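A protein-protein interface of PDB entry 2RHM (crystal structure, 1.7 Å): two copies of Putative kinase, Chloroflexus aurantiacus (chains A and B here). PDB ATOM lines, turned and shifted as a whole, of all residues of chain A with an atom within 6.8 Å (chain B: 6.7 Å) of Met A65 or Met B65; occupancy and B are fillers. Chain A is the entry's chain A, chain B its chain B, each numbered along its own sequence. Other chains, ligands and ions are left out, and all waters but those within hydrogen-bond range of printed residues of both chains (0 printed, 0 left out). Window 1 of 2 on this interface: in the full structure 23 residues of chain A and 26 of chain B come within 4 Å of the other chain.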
ATOM      1  N   LEU A  34      -8.617 -15.752 -16.262  1.00  0.00           N
ATOM      2  CA  LEU A  34      -7.953 -16.941 -15.801  1.00  0.00           C
ATOM      3  C   LEU A  34      -6.836 -17.187 -16.800  1.00  0.00           C
ATOM      4  O   LEU A  34      -7.108 -17.417 -17.971  1.00  0.00           O
ATOM      5  CB  LEU A  34      -8.923 -18.115 -15.785  1.00  0.00           C
ATOM      6  CG  LEU A  34     -10.186 -17.919 -14.948  1.00  0.00           C
ATOM      7  CD1 LEU A  34     -11.088 -19.148 -14.983  1.00  0.00           C
ATOM      8  CD2 LEU A  34      -9.825 -17.582 -13.522  1.00  0.00           C
ATOM      9  N   ALA A  38      -0.246 -17.332 -15.088  1.00  0.00           N
ATOM     10  CA  ALA A  38      -0.486 -16.752 -13.781  1.00  0.00           C
ATOM     11  C   ALA A  38      -0.728 -17.839 -12.722  1.00  0.00           C
ATOM     12  O   ALA A  38      -0.222 -17.736 -11.610  1.00  0.00           O
ATOM     13  CB  ALA A  38      -1.664 -15.808 -13.835  1.00  0.00           C
ATOM     14  N   PHE A  39      -1.492 -18.871 -13.071  1.00  0.00           N
ATOM     15  CA  PHE A  39      -1.727 -19.991 -12.148  1.00  0.00           C
ATOM     16  C   PHE A  39      -0.418 -20.734 -11.913  1.00  0.00           C
ATOM     17  O   PHE A  39      -0.111 -21.109 -10.796  1.00  0.00           O
ATOM     18  CB  PHE A  39      -2.761 -20.955 -12.718  1.00  0.00           C
ATOM     19  CG  PHE A  39      -4.196 -20.493 -12.582  1.00  0.00           C
ATOM     20  CD1 PHE A  39      -4.545 -19.156 -12.581  1.00  0.00           C
ATOM     21  CD2 PHE A  39      -5.207 -21.428 -12.507  1.00  0.00           C
ATOM     22  CE1 PHE A  39      -5.870 -18.763 -12.467  1.00  0.00           C
ATOM     23  CE2 PHE A  39      -6.532 -21.039 -12.397  1.00  0.00           C
ATOM     24  CZ  PHE A  39      -6.858 -19.709 -12.373  1.00  0.00           C
ATOM     25  N   LYS A  40       0.358 -20.942 -12.974  1.00  0.00           N
ATOM     26  CA  LYS A  40       1.656 -21.605 -12.831  1.00  0.00           C
ATOM     27  C   LYS A  40       2.560 -20.853 -11.852  1.00  0.00           C
ATOM     28  O   LYS A  40       3.242 -21.488 -11.036  1.00  0.00           O
ATOM     29  CB  LYS A  40       2.376 -21.712 -14.166  1.00  0.00           C
ATOM     30  CG  LYS A  40       1.824 -22.753 -15.127  1.00  0.00           C
ATOM     31  CD  LYS A  40       2.666 -22.830 -16.418  1.00  0.00           C
ATOM     32  CE  LYS A  40       4.066 -23.358 -16.154  1.00  0.00           C
ATOM     33  NZ  LYS A  40       4.770 -23.718 -17.415  1.00  0.00           N
ATOM     34  N   VAL A  42       1.710 -18.915  -9.302  1.00  0.00           N
ATOM     35  CA  VAL A  42       1.236 -19.109  -7.932  1.00  0.00           C
ATOM     36  C   VAL A  42       1.738 -20.466  -7.433  1.00  0.00           C
ATOM     37  O   VAL A  42       2.200 -20.593  -6.303  1.00  0.00           O
ATOM     38  CB  VAL A  42      -0.304 -19.014  -7.817  1.00  0.00           C
ATOM     39  CG1 VAL A  42      -0.778 -19.293  -6.377  1.00  0.00           C
ATOM     40  CG2 VAL A  42      -0.771 -17.640  -8.205  1.00  0.00           C
ATOM     41  N   MET A  43       1.651 -21.481  -8.277  1.00  0.00           N
ATOM     42  CA  MET A  43       2.112 -22.814  -7.891  1.00  0.00           C
ATOM     43  C   MET A  43       3.631 -22.927  -7.716  1.00  0.00           C
ATOM     44  O   MET A  43       4.085 -23.592  -6.801  1.00  0.00           O
ATOM     45  CB  MET A  43       1.594 -23.850  -8.877  1.00  0.00           C
ATOM     46  CG  MET A  43       0.123 -24.147  -8.629  1.00  0.00           C
ATOM     47  SD  MET A  43      -0.491 -25.567  -9.788  1.00  0.00           S
ATOM     48  CE  MET A  43      -0.567 -24.779 -10.942  1.00  0.00           C
ATOM     49  N   ALA A  60       0.411 -28.452 -16.624  1.00  0.00           N
ATOM     50  CA  ALA A  60      -0.752 -29.325 -16.829  1.00  0.00           C
ATOM     51  C   ALA A  60      -1.795 -29.144 -15.725  1.00  0.00           C
ATOM     52  O   ALA A  60      -3.002 -29.139 -15.975  1.00  0.00           O
ATOM     53  CB  ALA A  60      -0.301 -30.768 -16.890  1.00  0.00           C
ATOM     54  N   THR A  61      -1.309 -28.967 -14.505  1.00  0.00           N
ATOM     55  CA  THR A  61      -2.147 -28.791 -13.337  1.00  0.00           C
ATOM     56  C   THR A  61      -2.810 -27.427 -13.348  1.00  0.00           C
ATOM     57  O   THR A  61      -3.962 -27.293 -12.940  1.00  0.00           O
ATOM     58  CB  THR A  61      -1.319 -28.987 -12.069  1.00  0.00           C
ATOM     59  OG1 THR A  61      -0.715 -30.286 -12.114  1.00  0.00           O
ATOM     60  CG2 THR A  61      -2.157 -28.850 -10.830  1.00  0.00           C
ATOM     61  N   ALA A  62      -2.079 -26.414 -13.814  1.00  0.00           N
ATOM     62  CA  ALA A  62      -2.643 -25.057 -13.921  1.00  0.00           C
ATOM     63  C   ALA A  62      -3.821 -25.061 -14.897  1.00  0.00           C
ATOM     64  O   ALA A  62      -4.859 -24.443 -14.658  1.00  0.00           O
ATOM     65  CB  ALA A  62      -1.576 -24.079 -14.384  1.00  0.00           C
ATOM     66  N   ILE A  63      -3.654 -25.766 -16.009  1.00  0.00           N
ATOM     67  CA  ILE A  63      -4.719 -25.933 -16.985  1.00  0.00           C
ATOM     68  C   ILE A  63      -5.958 -26.567 -16.341  1.00  0.00           C
ATOM     69  O   ILE A  63      -7.064 -26.078 -16.541  1.00  0.00           O
ATOM     70  CB  ILE A  63      -4.216 -26.768 -18.209  1.00  0.00           C
ATOM     71  CG1 ILE A  63      -3.376 -25.869 -19.106  1.00  0.00           C
ATOM     72  CG2 ILE A  63      -5.367 -27.359 -19.015  1.00  0.00           C
ATOM     73  CD1 ILE A  63      -2.525 -26.617 -20.116  1.00  0.00           C
ATOM     74  N   MET A  64      -5.758 -27.646 -15.579  1.00  0.00           N
ATOM     75  CA  MET A  64      -6.847 -28.300 -14.848  1.00  0.00           C
ATOM     76  C   MET A  64      -7.522 -27.301 -13.895  1.00  0.00           C
ATOM     77  O   MET A  64      -8.745 -27.302 -13.743  1.00  0.00           O
ATOM     78  CB  MET A  64      -6.319 -29.498 -14.050  1.00  0.00           C
ATOM     79  CG  MET A  64      -5.850 -30.677 -14.892  1.00  0.00           C
ATOM     80  SD  MET A  64      -4.758 -31.949 -13.861  1.00  0.00           S
ATOM     81  CE  MET A  64      -5.661 -31.948 -12.253  1.00  0.00           C
ATOM     82  N   MET A  65      -6.715 -26.448 -13.262  1.00  0.00           N
ATOM     83  CA  MET A  65      -7.226 -25.410 -12.370  1.00  0.00           C
ATOM     84  C   MET A  65      -8.036 -24.388 -13.170  1.00  0.00           C
ATOM     85  O   MET A  65      -9.055 -23.894 -12.696  1.00  0.00           O
ATOM     86  CB  MET A  65      -6.091 -24.705 -11.611  1.00  0.00           C
ATOM     87  CG  MET A  65      -5.682 -25.363 -10.319  1.00  0.00           C
ATOM     88  SD  MET A  65      -7.184 -25.403  -9.001  1.00  0.00           S
ATOM     89  CE  MET A  65      -7.964 -23.773  -9.285  1.00  0.00           C
ATOM     90  N   LEU A  66      -7.577 -24.069 -14.382  1.00  0.00           N
ATOM     91  CA  LEU A  66      -8.336 -23.166 -15.269  1.00  0.00           C
ATOM     92  C   LEU A  66      -9.742 -23.693 -15.545  1.00  0.00           C
ATOM     93  O   LEU A  66     -10.712 -22.952 -15.454  1.00  0.00           O
ATOM     94  CB  LEU A  66      -7.607 -22.936 -16.614  1.00  0.00           C
ATOM     95  CG  LEU A  66      -7.098 -21.521 -16.911  1.00  0.00           C
ATOM     96  CD1 LEU A  66      -6.192 -20.998 -15.848  1.00  0.00           C
ATOM     97  CD2 LEU A  66      -6.387 -21.518 -18.272  1.00  0.00           C
ATOM     98  N   TYR A  67      -9.849 -24.970 -15.913  1.00  0.00           N
ATOM     99  CA  TYR A  67     -11.155 -25.547 -16.208  1.00  0.00           C
ATOM    100  C   TYR A  67     -12.020 -25.699 -14.962  1.00  0.00           C
ATOM    101  O   TYR A  67     -13.227 -25.518 -15.037  1.00  0.00           O
ATOM    102  CB  TYR A  67     -11.033 -26.874 -16.951  1.00  0.00           C
ATOM    103  CG  TYR A  67     -10.622 -26.697 -18.391  1.00  0.00           C
ATOM    104  CD1 TYR A  67     -11.548 -26.337 -19.369  1.00  0.00           C
ATOM    105  CD2 TYR A  67      -9.315 -26.892 -18.784  1.00  0.00           C
ATOM    106  CE1 TYR A  67     -11.168 -26.194 -20.697  1.00  0.00           C
ATOM    107  CE2 TYR A  67      -8.929 -26.740 -20.108  1.00  0.00           C
ATOM    108  CZ  TYR A  67      -9.850 -26.397 -21.058  1.00  0.00           C
ATOM    109  OH  TYR A  67      -9.436 -26.264 -22.375  1.00  0.00           O
ATOM    110  N   HIS A  68     -11.393 -26.014 -13.824  1.00  0.00           N
ATOM    111  CA  HIS A  68     -12.102 -26.125 -12.545  1.00  0.00           C
ATOM    112  C   HIS A  68     -12.764 -24.794 -12.182  1.00  0.00           C
ATOM    113  O   HIS A  68     -13.938 -24.750 -11.835  1.00  0.00           O
ATOM    114  CB  HIS A  68     -11.141 -26.551 -11.422  1.00  0.00           C
ATOM    115  CG  HIS A  68     -11.745 -26.482 -10.052  1.00  0.00           C
ATOM    116  ND1 HIS A  68     -12.576 -27.467  -9.552  1.00  0.00           N
ATOM    117  CD2 HIS A  68     -11.665 -25.531  -9.088  1.00  0.00           C
ATOM    118  CE1 HIS A  68     -12.960 -27.133  -8.333  1.00  0.00           C
ATOM    119  NE2 HIS A  68     -12.427 -25.961  -8.030  1.00  0.00           N
ATOM    120  N   THR A  69     -11.990 -23.718 -12.266  1.00  0.00           N
ATOM    121  CA  THR A  69     -12.454 -22.387 -11.906  1.00  0.00           C
ATOM    122  C   THR A  69     -13.476 -21.838 -12.912  1.00  0.00           C
ATOM    123  O   THR A  69     -14.484 -21.219 -12.529  1.00  0.00           O
ATOM    124  CB  THR A  69     -11.266 -21.410 -11.758  1.00  0.00           C
ATOM    125  OG1 THR A  69     -10.345 -21.902 -10.756  1.00  0.00           O
ATOM    126  CG2 THR A  69     -11.778 -20.054 -11.343  1.00  0.00           C
ATOM    127  N   ALA A  70     -13.204 -22.048 -14.192  1.00  0.00           N
ATOM    128  CA  ALA A  70     -14.122 -21.627 -15.257  1.00  0.00           C
ATOM    129  C   ALA A  70     -15.515 -22.195 -15.040  1.00  0.00           C
ATOM    130  O   ALA A  70     -16.516 -21.480 -15.173  1.00  0.00           O
ATOM    131  CB  ALA A  70     -13.603 -22.076 -16.589  1.00  0.00           C
ATOM    132  N   LEU B  34     -15.239 -21.122  -4.469  1.00  0.00           N
ATOM    133  CA  LEU B  34     -13.827 -21.479  -4.393  1.00  0.00           C
ATOM    134  C   LEU B  34     -13.551 -22.153  -3.065  1.00  0.00           C
ATOM    135  O   LEU B  34     -13.753 -21.557  -2.018  1.00  0.00           O
ATOM    136  CB  LEU B  34     -12.978 -20.228  -4.550  1.00  0.00           C
ATOM    137  CG  LEU B  34     -13.341 -19.300  -5.705  1.00  0.00           C
ATOM    138  CD1 LEU B  34     -12.464 -18.069  -5.598  1.00  0.00           C
ATOM    139  CD2 LEU B  34     -13.158 -19.957  -7.053  1.00  0.00           C
ATOM    140  N   ALA B  38     -11.068 -28.399  -2.543  1.00  0.00           N
ATOM    141  CA  ALA B  38     -11.292 -28.708  -3.971  1.00  0.00           C
ATOM    142  C   ALA B  38     -10.048 -28.354  -4.806  1.00  0.00           C
ATOM    143  O   ALA B  38      -9.644 -29.113  -5.684  1.00  0.00           O
ATOM    144  CB  ALA B  38     -12.536 -27.993  -4.504  1.00  0.00           C
ATOM    145  N   PHE B  39      -9.434 -27.216  -4.505  1.00  0.00           N
ATOM    146  CA  PHE B  39      -8.220 -26.773  -5.179  1.00  0.00           C
ATOM    147  C   PHE B  39      -7.061 -27.752  -4.889  1.00  0.00           C
ATOM    148  O   PHE B  39      -6.279 -28.097  -5.785  1.00  0.00           O
ATOM    149  CB  PHE B  39      -7.850 -25.346  -4.722  1.00  0.00           C
ATOM    150  CG  PHE B  39      -8.600 -24.239  -5.433  1.00  0.00           C
ATOM    151  CD1 PHE B  39      -9.927 -24.371  -5.820  1.00  0.00           C
ATOM    152  CD2 PHE B  39      -7.985 -23.024  -5.640  1.00  0.00           C
ATOM    153  CE1 PHE B  39     -10.583 -23.326  -6.465  1.00  0.00           C
ATOM    154  CE2 PHE B  39      -8.629 -21.987  -6.288  1.00  0.00           C
ATOM    155  CZ  PHE B  39      -9.926 -22.134  -6.691  1.00  0.00           C
ATOM    156  N   LYS B  40      -6.959 -28.203  -3.634  1.00  0.00           N
ATOM    157  CA  LYS B  40      -5.926 -29.147  -3.241  1.00  0.00           C
ATOM    158  C   LYS B  40      -6.067 -30.426  -4.047  1.00  0.00           C
ATOM    159  O   LYS B  40      -5.072 -30.958  -4.552  1.00  0.00           O
ATOM    160  CB  LYS B  40      -5.990 -29.480  -1.761  1.00  0.00           C
ATOM    161  CG  LYS B  40      -5.694 -28.316  -0.809  1.00  0.00           C
ATOM    162  CD  LYS B  40      -5.619 -28.781   0.674  1.00  0.00           C
ATOM    163  CE  LYS B  40      -4.511 -29.818   0.924  1.00  0.00           C
ATOM    164  NZ  LYS B  40      -4.463 -30.211   2.382  1.00  0.00           N
ATOM    165  N   VAL B  42      -7.462 -30.878  -7.030  1.00  0.00           N
ATOM    166  CA  VAL B  42      -7.038 -30.649  -8.408  1.00  0.00           C
ATOM    167  C   VAL B  42      -5.504 -30.763  -8.456  1.00  0.00           C
ATOM    168  O   VAL B  42      -4.951 -31.409  -9.336  1.00  0.00           O
ATOM    169  CB  VAL B  42      -7.495 -29.273  -8.936  1.00  0.00           C
ATOM    170  CG1 VAL B  42      -6.898 -29.003 -10.289  1.00  0.00           C
ATOM    171  CG2 VAL B  42      -9.025 -29.206  -9.011  1.00  0.00           C
ATOM    172  N   MET B  43      -4.815 -30.167  -7.485  1.00  0.00           N
ATOM    173  CA  MET B  43      -3.368 -30.265  -7.451  1.00  0.00           C
ATOM    174  C   MET B  43      -2.839 -31.670  -7.185  1.00  0.00           C
ATOM    175  O   MET B  43      -1.841 -32.058  -7.784  1.00  0.00           O
ATOM    176  CB  MET B  43      -2.768 -29.258  -6.481  1.00  0.00           C
ATOM    177  CG  MET B  43      -2.732 -27.895  -7.111  1.00  0.00           C
ATOM    178  SD  MET B  43      -1.836 -26.569  -5.988  1.00  0.00           S
ATOM    179  CE  MET B  43      -2.980 -26.395  -5.153  1.00  0.00           C
ATOM    180  N   ALA B  60      -1.119 -24.750   1.419  1.00  0.00           N
ATOM    181  CA  ALA B  60      -0.646 -23.367   1.432  1.00  0.00           C
ATOM    182  C   ALA B  60      -0.749 -22.755   0.021  1.00  0.00           C
ATOM    183  O   ALA B  60      -1.106 -21.575  -0.163  1.00  0.00           O
ATOM    184  CB  ALA B  60       0.794 -23.334   1.923  1.00  0.00           C
ATOM    185  N   THR B  61      -0.475 -23.586  -0.976  1.00  0.00           N
ATOM    186  CA  THR B  61      -0.525 -23.156  -2.369  1.00  0.00           C
ATOM    187  C   THR B  61      -1.980 -22.971  -2.807  1.00  0.00           C
ATOM    188  O   THR B  61      -2.318 -21.982  -3.467  1.00  0.00           O
ATOM    189  CB  THR B  61       0.217 -24.139  -3.291  1.00  0.00           C
ATOM    190  OG1 THR B  61       1.566 -24.292  -2.846  1.00  0.00           O
ATOM    191  CG2 THR B  61       0.256 -23.613  -4.708  1.00  0.00           C
ATOM    192  N   ALA B  62      -2.838 -23.911  -2.415  1.00  0.00           N
ATOM    193  CA  ALA B  62      -4.271 -23.820  -2.715  1.00  0.00           C
ATOM    194  C   ALA B  62      -4.862 -22.527  -2.139  1.00  0.00           C
ATOM    195  O   ALA B  62      -5.641 -21.854  -2.800  1.00  0.00           O
ATOM    196  CB  ALA B  62      -5.007 -25.027  -2.172  1.00  0.00           C
ATOM    197  N   ILE B  63      -4.470 -22.173  -0.924  1.00  0.00           N
ATOM    198  CA  ILE B  63      -4.929 -20.927  -0.304  1.00  0.00           C
ATOM    199  C   ILE B  63      -4.520 -19.704  -1.152  1.00  0.00           C
ATOM    200  O   ILE B  63      -5.334 -18.828  -1.398  1.00  0.00           O
ATOM    201  CB  ILE B  63      -4.419 -20.789   1.155  1.00  0.00           C
ATOM    202  CG1 ILE B  63      -5.136 -21.791   2.065  1.00  0.00           C
ATOM    203  CG2 ILE B  63      -4.665 -19.394   1.672  1.00  0.00           C
ATOM    204  CD1 ILE B  63      -4.437 -22.015   3.388  1.00  0.00           C
ATOM    205  N   MET B  64      -3.271 -19.706  -1.633  1.00  0.00           N
ATOM    206  CA  MET B  64      -2.772 -18.704  -2.585  1.00  0.00           C
ATOM    207  C   MET B  64      -3.629 -18.659  -3.870  1.00  0.00           C
ATOM    208  O   MET B  64      -3.931 -17.575  -4.380  1.00  0.00           O
ATOM    209  CB  MET B  64      -1.294 -18.973  -2.945  1.00  0.00           C
ATOM    210  CG  MET B  64      -0.297 -18.703  -1.817  1.00  0.00           C
ATOM    211  SD  MET B  64       1.547 -19.422  -2.095  1.00  0.00           S
ATOM    212  CE  MET B  64       1.841 -19.037  -3.855  1.00  0.00           C
ATOM    213  N   MET B  65      -4.008 -19.820  -4.406  1.00  0.00           N
ATOM    214  CA  MET B  65      -4.863 -19.863  -5.598  1.00  0.00           C
ATOM    215  C   MET B  65      -6.244 -19.297  -5.298  1.00  0.00           C
ATOM    216  O   MET B  65      -6.876 -18.658  -6.148  1.00  0.00           O
ATOM    217  CB  MET B  65      -5.009 -21.306  -6.109  1.00  0.00           C
ATOM    218  CG  MET B  65      -3.954 -21.742  -7.076  1.00  0.00           C
ATOM    219  SD  MET B  65      -3.922 -20.607  -8.653  1.00  0.00           S
ATOM    220  CE  MET B  65      -5.681 -20.734  -9.240  1.00  0.00           C
ATOM    221  N   LEU B  66      -6.731 -19.565  -4.094  1.00  0.00           N
ATOM    222  CA  LEU B  66      -8.048 -19.104  -3.672  1.00  0.00           C
ATOM    223  C   LEU B  66      -8.103 -17.562  -3.716  1.00  0.00           C
ATOM    224  O   LEU B  66      -9.011 -16.976  -4.302  1.00  0.00           O
ATOM    225  CB  LEU B  66      -8.328 -19.601  -2.246  1.00  0.00           C
ATOM    226  CG  LEU B  66      -9.657 -20.328  -2.020  1.00  0.00           C
ATOM    227  CD1 LEU B  66      -9.750 -21.493  -2.923  1.00  0.00           C
ATOM    228  CD2 LEU B  66      -9.751 -20.780  -0.575  1.00  0.00           C
ATOM    229  N   TYR B  67      -7.124 -16.912  -3.105  1.00  0.00           N
ATOM    230  CA  TYR B  67      -7.051 -15.450  -3.099  1.00  0.00           C
ATOM    231  C   TYR B  67      -6.791 -14.851  -4.492  1.00  0.00           C
ATOM    232  O   TYR B  67      -7.334 -13.806  -4.828  1.00  0.00           O
ATOM    233  CB  TYR B  67      -5.999 -14.961  -2.115  1.00  0.00           C
ATOM    234  CG  TYR B  67      -6.456 -15.057  -0.681  1.00  0.00           C
ATOM    235  CD1 TYR B  67      -7.336 -14.131  -0.148  1.00  0.00           C
ATOM    236  CD2 TYR B  67      -6.052 -16.099   0.123  1.00  0.00           C
ATOM    237  CE1 TYR B  67      -7.784 -14.225   1.163  1.00  0.00           C
ATOM    238  CE2 TYR B  67      -6.479 -16.190   1.447  1.00  0.00           C
ATOM    239  CZ  TYR B  67      -7.341 -15.262   1.960  1.00  0.00           C
ATOM    240  OH  TYR B  67      -7.753 -15.391   3.284  1.00  0.00           O
ATOM    241  N   HIS B  68      -5.988 -15.537  -5.300  1.00  0.00           N
ATOM    242  CA  HIS B  68      -5.689 -15.078  -6.668  1.00  0.00           C
ATOM    243  C   HIS B  68      -6.963 -15.076  -7.524  1.00  0.00           C
ATOM    244  O   HIS B  68      -7.286 -14.107  -8.222  1.00  0.00           O
ATOM    245  CB  HIS B  68      -4.633 -15.987  -7.321  1.00  0.00           C
ATOM    246  CG  HIS B  68      -4.451 -15.734  -8.789  1.00  0.00           C
ATOM    247  ND1 HIS B  68      -3.707 -14.681  -9.272  1.00  0.00           N
ATOM    248  CD2 HIS B  68      -4.931 -16.388  -9.877  1.00  0.00           C
ATOM    249  CE1 HIS B  68      -3.735 -14.692 -10.592  1.00  0.00           C
ATOM    250  NE2 HIS B  68      -4.457 -15.729 -10.988  1.00  0.00           N
ATOM    251  N   THR B  69      -7.698 -16.174  -7.437  1.00  0.00           N
ATOM    252  CA  THR B  69      -8.900 -16.353  -8.249  1.00  0.00           C
ATOM    253  C   THR B  69     -10.001 -15.426  -7.726  1.00  0.00           C
ATOM    254  O   THR B  69     -10.750 -14.805  -8.500  1.00  0.00           O
ATOM    255  CB  THR B  69      -9.320 -17.828  -8.244  1.00  0.00           C
ATOM    256  OG1 THR B  69      -8.278 -18.606  -8.856  1.00  0.00           O
ATOM    257  CG2 THR B  69     -10.575 -18.022  -9.038  1.00  0.00           C
ATOM    258  N   ALA B  70     -10.094 -15.305  -6.420  1.00  0.00           N
ATOM    259  CA  ALA B  70     -11.088 -14.388  -5.818  1.00  0.00           C
ATOM    260  C   ALA B  70     -10.941 -12.958  -6.298  1.00  0.00           C
ATOM    261  O   ALA B  70     -11.928 -12.254  -6.503  1.00  0.00           O
ATOM    262  CB  ALA B  70     -11.004 -14.414  -4.314  1.00  0.00           C
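Hydrophobic or aromatic side chains of chain B that line the printed part of chain A: Ala B38, Phe B39, Val B42, Met B43, Met B64, Met B65 and His B68. Along chain B the printed residues that touch a printed residue of chain A span positions 38 to 69. Printed residues of chain A that touch a printed residue of chain B: Ala A38, Phe A39, Val A42, Met A43, Thr A61, Met A64, Met A65, His A68 and Thr A69. Hydrophobic or aromatic side chains of chain A that line the printed part of chain B: Ala A38, Phe A39, Val A42, Met A43, Met A64, Met A65 and His A68. Among the printed residues, 17 pairs touch across the chains. Among the printed residues, no Asp or Glu carboxylate lies within 4 Å of a Lys or Arg side-chain nitrogen of the other chain.
Val A42 touches Thr B61, but with the chains exchanged Thr A61 does not touch Val B42 (4.1 Å). Val A42 touches Met B65, and with the chains exchanged Met A65 touches Val B42. Met A43 touches Thr B61, and with the chains exchanged Thr A61 touches Met B43. Met B65 touches its own counterpart, Met A65. Positions printed for both chains: 34, 38, 39, 40, 42, 43, 60, 61, 62, 63, 64, 65, 66, 67, 68, 69 and 70. Of the 17 pairs that touch across the chains among the printed residues, 14 have their exchanged pair printed and touching as well.
Printed residues of chain B within 4 Å of Met A65: Phe B39, Val B42 and Met B65. Of the printed residues of chain A, Met B65 touches Phe A39, Val A42 and Met A65. Of the printed residues of chain A, Phe B39 touches Met A65 (3.6 Å) and His A68 (3.6 Å). Printed residues of chain A within 4 Å of Val B42: Met A64, Met A65 and His A68. Printed residues of chain B within 4 Å of Met A43: Thr B61 (3.8 Å). Of the printed residues of chain B, Val A42 touches Thr B61, Met B64 and Met B65. Leu A66 touches none of the printed residues of chain B. Ala B62 touches none of the printed residues of chain A.
The backbone carbonyl oxygen (O) of Met B65 is in hydrogen-bond range of the side-chain hydroxyl (OG1) of Thr B69. O of Met A65 is in hydrogen-bond range of OG1 of Thr A69 (3.1 Å).
Among the printed residues, pairs that only touch across the chains: Ala A38 with His B68 (3.99 Å), Phe A39 with Met B65 (3.3 Å), Phe A39 with His B68 (3.6 Å), Phe A39 with Thr B69 (3.9 Å), Val A42 with Thr B61 (3.9 Å), Val A42 with Met B64 (2.9 Å), Val A42 with Met B65 (3.8 Å), Met A43 with Thr B61 (3.8 Å), Thr A61 with Met B43 (3.9 Å), Met A64 with Val B42 (3.1 Å), Met A65 with Phe B39 (3.6 Å), Met A65 with Val B42 (3.8 Å), Met A65 with Met B65 (3.8 Å), His A68 with Ala B38 (3.9 Å), His A68 with Phe B39 (3.6 Å), His A68 with Val B42 (3.99 Å) and Thr A69 with Thr B69 (3.3 Å).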
